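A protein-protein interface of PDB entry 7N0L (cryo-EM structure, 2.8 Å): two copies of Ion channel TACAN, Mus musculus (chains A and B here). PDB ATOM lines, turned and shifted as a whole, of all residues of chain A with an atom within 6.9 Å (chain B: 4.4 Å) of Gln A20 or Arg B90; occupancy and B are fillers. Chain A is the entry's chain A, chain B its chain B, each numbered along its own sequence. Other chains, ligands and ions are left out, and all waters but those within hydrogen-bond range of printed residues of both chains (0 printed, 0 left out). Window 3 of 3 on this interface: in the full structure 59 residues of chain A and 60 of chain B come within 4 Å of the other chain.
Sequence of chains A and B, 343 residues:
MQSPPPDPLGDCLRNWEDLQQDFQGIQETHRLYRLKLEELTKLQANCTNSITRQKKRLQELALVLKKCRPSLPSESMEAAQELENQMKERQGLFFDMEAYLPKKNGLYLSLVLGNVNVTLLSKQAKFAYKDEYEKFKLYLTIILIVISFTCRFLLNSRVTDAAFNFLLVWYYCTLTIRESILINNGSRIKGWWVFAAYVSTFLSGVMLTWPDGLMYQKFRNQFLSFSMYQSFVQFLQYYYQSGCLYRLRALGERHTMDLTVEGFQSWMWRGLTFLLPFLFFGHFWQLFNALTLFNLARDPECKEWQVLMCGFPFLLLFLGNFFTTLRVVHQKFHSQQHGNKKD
NE2 of Gln B54 lies close to O of Leu A19 (2.4 Å). The side-chain amide oxygen of Gln B54 lies close to the side-chain carboxylate of Asp A22 (2.8 Å). The side-chain amide oxygen (OE1) of Gln B86 is in hydrogen-bond range of the indole nitrogen (NE1) of Trp A16, at 2.7 Å.
NE2 of Gln A20 is in hydrogen-bond range of O of Glu A17 (3.1 Å). O of Gln A20 lies close to OE1 of Gln A24 (2.9 Å). The indole nitrogen (NE1) of Trp A16 sits close to the side-chain carboxylate (OE1) of Glu A17 (3.4 Å).
Among the printed residues, pairs that only touch across the chains: Trp A16 with Met B87 (3.5 Å), Trp A16 with Arg B90 (3.2 Å), Gln A20 with Arg B90 (3.2 Å), Phe A23 with Gln B54 (3.7 Å), Phe A23 with Arg B90 (3.1 Å), Phe A23 with Leu B93 (3.5 Å) and Phe A23 with Phe B94 (3.5 Å).
Of the printed residues of chain B, Trp A16 touches Gln B86 (2.7 Å), Met B87 (3.5 Å) and Arg B90 (3.2 Å). Printed residues of chain B within 4 Å of Phe A23: Gln B54 (3.7 Å), Arg B90 (3.1 Å), Leu B93 (3.5 Å) and Phe B94 (3.5 Å). Of the printed residues of chain A, Gln B54 touches Leu A19, Asp A22 and Phe A23. Of chain A, only Trp A16 (3.2 Å), Gln A20 (3.2 Å) and Phe A23 (3.1 Å) come within 4 Å of Arg B90. The nearest residue of chain B that does not touch Gln A20 is Gln B54 (4.1 Å). The nearest printed residue of chain A that does not touch Gln B54 is Gln A20 (4.1 Å).
Printed residues of chain B that touch a printed residue of chain A: Gln B54, Gln B86, Met B87, Arg B90, Leu B93 and Phe B94. Hydrophobic or aromatic side chains of chain B that line the printed part of chain A: Met B87, Leu B93 and Phe B94. Hydrophobic or aromatic side chains of chain A within 4 Å of the printed part of chain B: Trp A16 and Phe A23. Among the printed residues, 10 pairs touch across the chains. Among the printed residues, no Asp or Glu carboxylate lies within 4 Å of a Lys or Arg side-chain nitrogen of the other chain.
No position is printed for both chains.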
ATOM      1  N   ASN A  15       6.614 -21.477   9.834  1.00  0.00           N
ATOM      2  CA  ASN A  15       7.286 -20.669   8.826  1.00  0.00           C
ATOM      3  C   ASN A  15       7.527 -21.442   7.538  1.00  0.00           C
ATOM      4  O   ASN A  15       7.731 -20.824   6.488  1.00  0.00           O
ATOM      5  CB  ASN A  15       8.616 -20.141   9.368  1.00  0.00           C
ATOM      6  CG  ASN A  15       9.197 -19.033   8.510  1.00  0.00           C
ATOM      7  OD1 ASN A  15       8.464 -18.225   7.939  1.00  0.00           O
ATOM      8  ND2 ASN A  15      10.520 -18.991   8.415  1.00  0.00           N
ATOM      9  N   TRP A  16       7.506 -22.774   7.598  1.00  0.00           N
ATOM     10  CA  TRP A  16       7.629 -23.575   6.386  1.00  0.00           C
ATOM     11  C   TRP A  16       6.411 -23.414   5.489  1.00  0.00           C
ATOM     12  O   TRP A  16       6.538 -23.455   4.260  1.00  0.00           O
ATOM     13  CB  TRP A  16       7.825 -25.045   6.751  1.00  0.00           C
ATOM     14  CG  TRP A  16       7.608 -25.988   5.615  1.00  0.00           C
ATOM     15  CD1 TRP A  16       6.553 -26.834   5.441  1.00  0.00           C
ATOM     16  CD2 TRP A  16       8.483 -26.207   4.504  1.00  0.00           C
ATOM     17  NE1 TRP A  16       6.710 -27.554   4.284  1.00  0.00           N
ATOM     18  CE2 TRP A  16       7.889 -27.189   3.690  1.00  0.00           C
ATOM     19  CE3 TRP A  16       9.709 -25.662   4.115  1.00  0.00           C
ATOM     20  CZ2 TRP A  16       8.477 -27.637   2.511  1.00  0.00           C
ATOM     21  CZ3 TRP A  16      10.291 -26.107   2.948  1.00  0.00           C
ATOM     22  CH2 TRP A  16       9.677 -27.086   2.160  1.00  0.00           C
ATOM     23  N   GLU A  17       5.232 -23.226   6.079  1.00  0.00           N
ATOM     24  CA  GLU A  17       4.009 -23.074   5.304  1.00  0.00           C
ATOM     25  C   GLU A  17       3.726 -21.629   4.928  1.00  0.00           C
ATOM     26  O   GLU A  17       3.132 -21.376   3.874  1.00  0.00           O
ATOM     27  CB  GLU A  17       2.823 -23.652   6.079  1.00  0.00           C
ATOM     28  CG  GLU A  17       3.032 -25.091   6.498  1.00  0.00           C
ATOM     29  CD  GLU A  17       2.875 -26.052   5.339  1.00  0.00           C
ATOM     30  OE1 GLU A  17       3.506 -27.129   5.367  1.00  0.00           O
ATOM     31  OE2 GLU A  17       2.120 -25.729   4.400  1.00  0.00           O
ATOM     32  N   ASP A  18       4.139 -20.673   5.763  1.00  0.00           N
ATOM     33  CA  ASP A  18       4.013 -19.268   5.399  1.00  0.00           C
ATOM     34  C   ASP A  18       4.939 -18.890   4.252  1.00  0.00           C
ATOM     35  O   ASP A  18       4.749 -17.835   3.638  1.00  0.00           O
ATOM     36  CB  ASP A  18       4.291 -18.380   6.611  1.00  0.00           C
ATOM     37  CG  ASP A  18       3.399 -17.156   6.651  1.00  0.00           C
ATOM     38  OD1 ASP A  18       3.459 -16.342   5.705  1.00  0.00           O
ATOM     39  OD2 ASP A  18       2.635 -17.008   7.627  1.00  0.00           O
ATOM     40  N   LEU A  19       5.935 -19.724   3.951  1.00  0.00           N
ATOM     41  CA  LEU A  19       6.812 -19.490   2.815  1.00  0.00           C
ATOM     42  C   LEU A  19       6.346 -20.208   1.558  1.00  0.00           C
ATOM     43  O   LEU A  19       6.754 -19.826   0.456  1.00  0.00           O
ATOM     44  CB  LEU A  19       8.243 -19.921   3.149  1.00  0.00           C
ATOM     45  N   GLN A  20       5.508 -21.235   1.695  1.00  0.00           N
ATOM     46  CA  GLN A  20       4.913 -21.913   0.554  1.00  0.00           C
ATOM     47  C   GLN A  20       3.462 -21.517   0.333  1.00  0.00           C
ATOM     48  O   GLN A  20       2.787 -22.117  -0.509  1.00  0.00           O
ATOM     49  CB  GLN A  20       5.027 -23.430   0.712  1.00  0.00           C
ATOM     50  CG  GLN A  20       4.324 -23.999   1.925  1.00  0.00           C
ATOM     51  CD  GLN A  20       2.899 -24.428   1.639  1.00  0.00           C
ATOM     52  OE1 GLN A  20       2.663 -25.491   1.065  1.00  0.00           O
ATOM     53  NE2 GLN A  20       1.940 -23.607   2.048  1.00  0.00           N
ATOM     54  N   GLN A  21       2.960 -20.532   1.080  1.00  0.00           N
ATOM     55  CA  GLN A  21       1.680 -19.928   0.730  1.00  0.00           C
ATOM     56  C   GLN A  21       1.763 -19.198  -0.601  1.00  0.00           C
ATOM     57  O   GLN A  21       0.731 -18.975  -1.243  1.00  0.00           O
ATOM     58  CB  GLN A  21       1.222 -18.972   1.832  1.00  0.00           C
ATOM     59  N   ASP A  22       2.969 -18.820  -1.023  1.00  0.00           N
ATOM     60  CA  ASP A  22       3.202 -18.235  -2.331  1.00  0.00           C
ATOM     61  C   ASP A  22       3.928 -19.172  -3.285  1.00  0.00           C
ATOM     62  O   ASP A  22       4.030 -18.856  -4.474  1.00  0.00           O
ATOM     63  CB  ASP A  22       4.003 -16.931  -2.197  1.00  0.00           C
ATOM     64  CG  ASP A  22       5.362 -17.148  -1.573  1.00  0.00           C
ATOM     65  OD1 ASP A  22       5.495 -16.949  -0.346  1.00  0.00           O
ATOM     66  OD2 ASP A  22       6.300 -17.519  -2.309  1.00  0.00           O
ATOM     67  N   PHE A  23       4.441 -20.308  -2.801  1.00  0.00           N
ATOM     68  CA  PHE A  23       5.001 -21.299  -3.710  1.00  0.00           C
ATOM     69  C   PHE A  23       3.928 -21.940  -4.572  1.00  0.00           C
ATOM     70  O   PHE A  23       4.243 -22.460  -5.648  1.00  0.00           O
ATOM     71  CB  PHE A  23       5.751 -22.382  -2.939  1.00  0.00           C
ATOM     72  CG  PHE A  23       6.466 -23.361  -3.819  1.00  0.00           C
ATOM     73  CD1 PHE A  23       7.378 -22.927  -4.764  1.00  0.00           C
ATOM     74  CD2 PHE A  23       6.219 -24.718  -3.712  1.00  0.00           C
ATOM     75  CE1 PHE A  23       8.036 -23.826  -5.576  1.00  0.00           C
ATOM     76  CE2 PHE A  23       6.875 -25.623  -4.521  1.00  0.00           C
ATOM     77  CZ  PHE A  23       7.785 -25.176  -5.455  1.00  0.00           C
ATOM     78  N   GLN A  24       2.674 -21.930  -4.118  1.00  0.00           N
ATOM     79  CA  GLN A  24       1.570 -22.220  -5.022  1.00  0.00           C
ATOM     80  C   GLN A  24       1.372 -21.084  -6.015  1.00  0.00           C
ATOM     81  O   GLN A  24       0.852 -21.303  -7.113  1.00  0.00           O
ATOM     82  CB  GLN A  24       0.286 -22.470  -4.232  1.00  0.00           C
ATOM     83  CG  GLN A  24       0.457 -23.395  -3.038  1.00  0.00           C
ATOM     84  CD  GLN A  24      -0.251 -22.884  -1.798  1.00  0.00           C
ATOM     85  OE1 GLN A  24       0.030 -21.787  -1.316  1.00  0.00           O
ATOM     86  NE2 GLN A  24      -1.172 -23.682  -1.271  1.00  0.00           N
ATOM     87  N   GLY A  25       1.781 -19.872  -5.645  1.00  0.00           N
ATOM     88  CA  GLY A  25       1.631 -18.713  -6.500  1.00  0.00           C
ATOM     89  C   GLY A  25       2.634 -18.665  -7.631  1.00  0.00           C
ATOM     90  O   GLY A  25       2.249 -18.470  -8.787  1.00  0.00           O
ATOM     91  N   GLN B  54      12.973 -16.610  -2.424  1.00  0.00           N
ATOM     92  CA  GLN B  54      12.413 -17.709  -1.646  1.00  0.00           C
ATOM     93  C   GLN B  54      13.455 -18.788  -1.390  1.00  0.00           C
ATOM     94  O   GLN B  54      13.503 -19.364  -0.298  1.00  0.00           O
ATOM     95  CB  GLN B  54      11.201 -18.301  -2.362  1.00  0.00           C
ATOM     96  CG  GLN B  54      10.523 -19.415  -1.583  1.00  0.00           C
ATOM     97  CD  GLN B  54       9.065 -19.578  -1.948  1.00  0.00           C
ATOM     98  OE1 GLN B  54       8.576 -18.953  -2.887  1.00  0.00           O
ATOM     99  NE2 GLN B  54       8.360 -20.419  -1.202  1.00  0.00           N
ATOM    100  N   GLN B  86      10.935 -32.483   2.277  1.00  0.00           N
ATOM    101  CA  GLN B  86       9.959 -31.478   1.879  1.00  0.00           C
ATOM    102  C   GLN B  86      10.610 -30.293   1.179  1.00  0.00           C
ATOM    103  O   GLN B  86       9.979 -29.664   0.323  1.00  0.00           O
ATOM    104  CB  GLN B  86       9.170 -31.001   3.099  1.00  0.00           C
ATOM    105  CG  GLN B  86       7.936 -31.832   3.399  1.00  0.00           C
ATOM    106  CD  GLN B  86       6.709 -30.982   3.667  1.00  0.00           C
ATOM    107  OE1 GLN B  86       6.488 -29.965   3.011  1.00  0.00           O
ATOM    108  NE2 GLN B  86       5.902 -31.396   4.638  1.00  0.00           N
ATOM    109  N   MET B  87      11.857 -29.964   1.521  1.00  0.00           N
ATOM    110  CA  MET B  87      12.572 -28.884   0.856  1.00  0.00           C
ATOM    111  C   MET B  87      13.719 -29.388  -0.010  1.00  0.00           C
ATOM    112  O   MET B  87      14.448 -28.577  -0.590  1.00  0.00           O
ATOM    113  CB  MET B  87      13.089 -27.863   1.876  1.00  0.00           C
ATOM    114  CG  MET B  87      13.762 -28.424   3.124  1.00  0.00           C
ATOM    115  SD  MET B  87      15.318 -29.290   2.840  1.00  0.00           S
ATOM    116  CE  MET B  87      16.322 -27.982   2.143  1.00  0.00           C
ATOM    117  N   LYS B  88      13.899 -30.704  -0.118  1.00  0.00           N
ATOM    118  CA  LYS B  88      14.898 -31.219  -1.047  1.00  0.00           C
ATOM    119  C   LYS B  88      14.347 -31.276  -2.465  1.00  0.00           C
ATOM    120  O   LYS B  88      15.056 -30.953  -3.423  1.00  0.00           O
ATOM    121  CB  LYS B  88      15.382 -32.599  -0.602  1.00  0.00           C
ATOM    122  CG  LYS B  88      16.275 -33.291  -1.621  1.00  0.00           C
ATOM    123  CD  LYS B  88      17.383 -34.083  -0.952  1.00  0.00           C
ATOM    124  CE  LYS B  88      18.552 -34.299  -1.901  1.00  0.00           C
ATOM    125  NZ  LYS B  88      19.831 -33.773  -1.346  1.00  0.00           N
ATOM    126  N   GLU B  89      13.084 -31.676  -2.612  1.00  0.00           N
ATOM    127  CA  GLU B  89      12.453 -31.669  -3.926  1.00  0.00           C
ATOM    128  C   GLU B  89      12.011 -30.265  -4.324  1.00  0.00           C
ATOM    129  O   GLU B  89      12.043 -29.917  -5.509  1.00  0.00           O
ATOM    130  CB  GLU B  89      11.276 -32.647  -3.947  1.00  0.00           C
ATOM    131  CG  GLU B  89      10.099 -32.263  -3.062  1.00  0.00           C
ATOM    132  CD  GLU B  89       9.089 -31.390  -3.778  1.00  0.00           C
ATOM    133  OE1 GLU B  89       8.186 -30.849  -3.107  1.00  0.00           O
ATOM    134  OE2 GLU B  89       9.199 -31.247  -5.013  1.00  0.00           O
ATOM    135  N   ARG B  90      11.588 -29.447  -3.354  1.00  0.00           N
ATOM    136  CA  ARG B  90      11.188 -28.079  -3.668  1.00  0.00           C
ATOM    137  C   ARG B  90      12.375 -27.259  -4.152  1.00  0.00           C
ATOM    138  O   ARG B  90      12.281 -26.543  -5.154  1.00  0.00           O
ATOM    139  CB  ARG B  90      10.537 -27.415  -2.456  1.00  0.00           C
ATOM    140  CG  ARG B  90      10.332 -25.921  -2.652  1.00  0.00           C
ATOM    141  CD  ARG B  90       9.523 -25.308  -1.531  1.00  0.00           C
ATOM    142  NE  ARG B  90       8.149 -25.794  -1.543  1.00  0.00           N
ATOM    143  CZ  ARG B  90       7.320 -25.709  -0.510  1.00  0.00           C
ATOM    144  NH1 ARG B  90       6.086 -26.183  -0.606  1.00  0.00           N
ATOM    145  NH2 ARG B  90       7.726 -25.148   0.619  1.00  0.00           N
ATOM    146  N   GLN B  91      13.499 -27.329  -3.434  1.00  0.00           N
ATOM    147  CA  GLN B  91      14.719 -26.708  -3.940  1.00  0.00           C
ATOM    148  C   GLN B  91      15.107 -27.295  -5.288  1.00  0.00           C
ATOM    149  O   GLN B  91      15.708 -26.605  -6.120  1.00  0.00           O
ATOM    150  CB  GLN B  91      15.854 -26.871  -2.930  1.00  0.00           C
ATOM    151  CG  GLN B  91      17.191 -26.310  -3.389  1.00  0.00           C
ATOM    152  CD  GLN B  91      18.367 -27.135  -2.907  1.00  0.00           C
ATOM    153  OE1 GLN B  91      19.435 -27.133  -3.520  1.00  0.00           O
ATOM    154  NE2 GLN B  91      18.177 -27.846  -1.801  1.00  0.00           N
ATOM    155  N   GLY B  92      14.764 -28.564  -5.526  1.00  0.00           N
ATOM    156  CA  GLY B  92      14.863 -29.125  -6.859  1.00  0.00           C
ATOM    157  C   GLY B  92      13.744 -28.707  -7.783  1.00  0.00           C
ATOM    158  O   GLY B  92      13.931 -28.710  -9.004  1.00  0.00           O
ATOM    159  N   LEU B  93      12.581 -28.354  -7.230  1.00  0.00           N
ATOM    160  CA  LEU B  93      11.526 -27.767  -8.048  1.00  0.00           C
ATOM    161  C   LEU B  93      11.935 -26.388  -8.543  1.00  0.00           C
ATOM    162  O   LEU B  93      11.634 -26.014  -9.681  1.00  0.00           O
ATOM    163  CB  LEU B  93      10.222 -27.680  -7.258  1.00  0.00           C
ATOM    164  CG  LEU B  93       9.283 -28.887  -7.259  1.00  0.00           C
ATOM    165  CD1 LEU B  93       7.933 -28.501  -6.680  1.00  0.00           C
ATOM    166  CD2 LEU B  93       9.124 -29.459  -8.655  1.00  0.00           C
ATOM    167  N   PHE B  94      12.615 -25.616  -7.692  1.00  0.00           N
ATOM    168  CA  PHE B  94      13.161 -24.338  -8.129  1.00  0.00           C
ATOM    169  C   PHE B  94      14.172 -24.523  -9.251  1.00  0.00           C
ATOM    170  O   PHE B  94      14.309 -23.649 -10.113  1.00  0.00           O
ATOM    171  CB  PHE B  94      13.805 -23.611  -6.949  1.00  0.00           C
ATOM    172  CG  PHE B  94      12.817 -23.001  -5.997  1.00  0.00           C
ATOM    173  CD1 PHE B  94      11.740 -22.274  -6.467  1.00  0.00           C
ATOM    174  CD2 PHE B  94      12.972 -23.150  -4.629  1.00  0.00           C
ATOM    175  CE1 PHE B  94      10.835 -21.709  -5.589  1.00  0.00           C
ATOM    176  CE2 PHE B  94      12.071 -22.590  -3.750  1.00  0.00           C
ATOM    177  CZ  PHE B  94      11.000 -21.869  -4.231  1.00  0.00           C
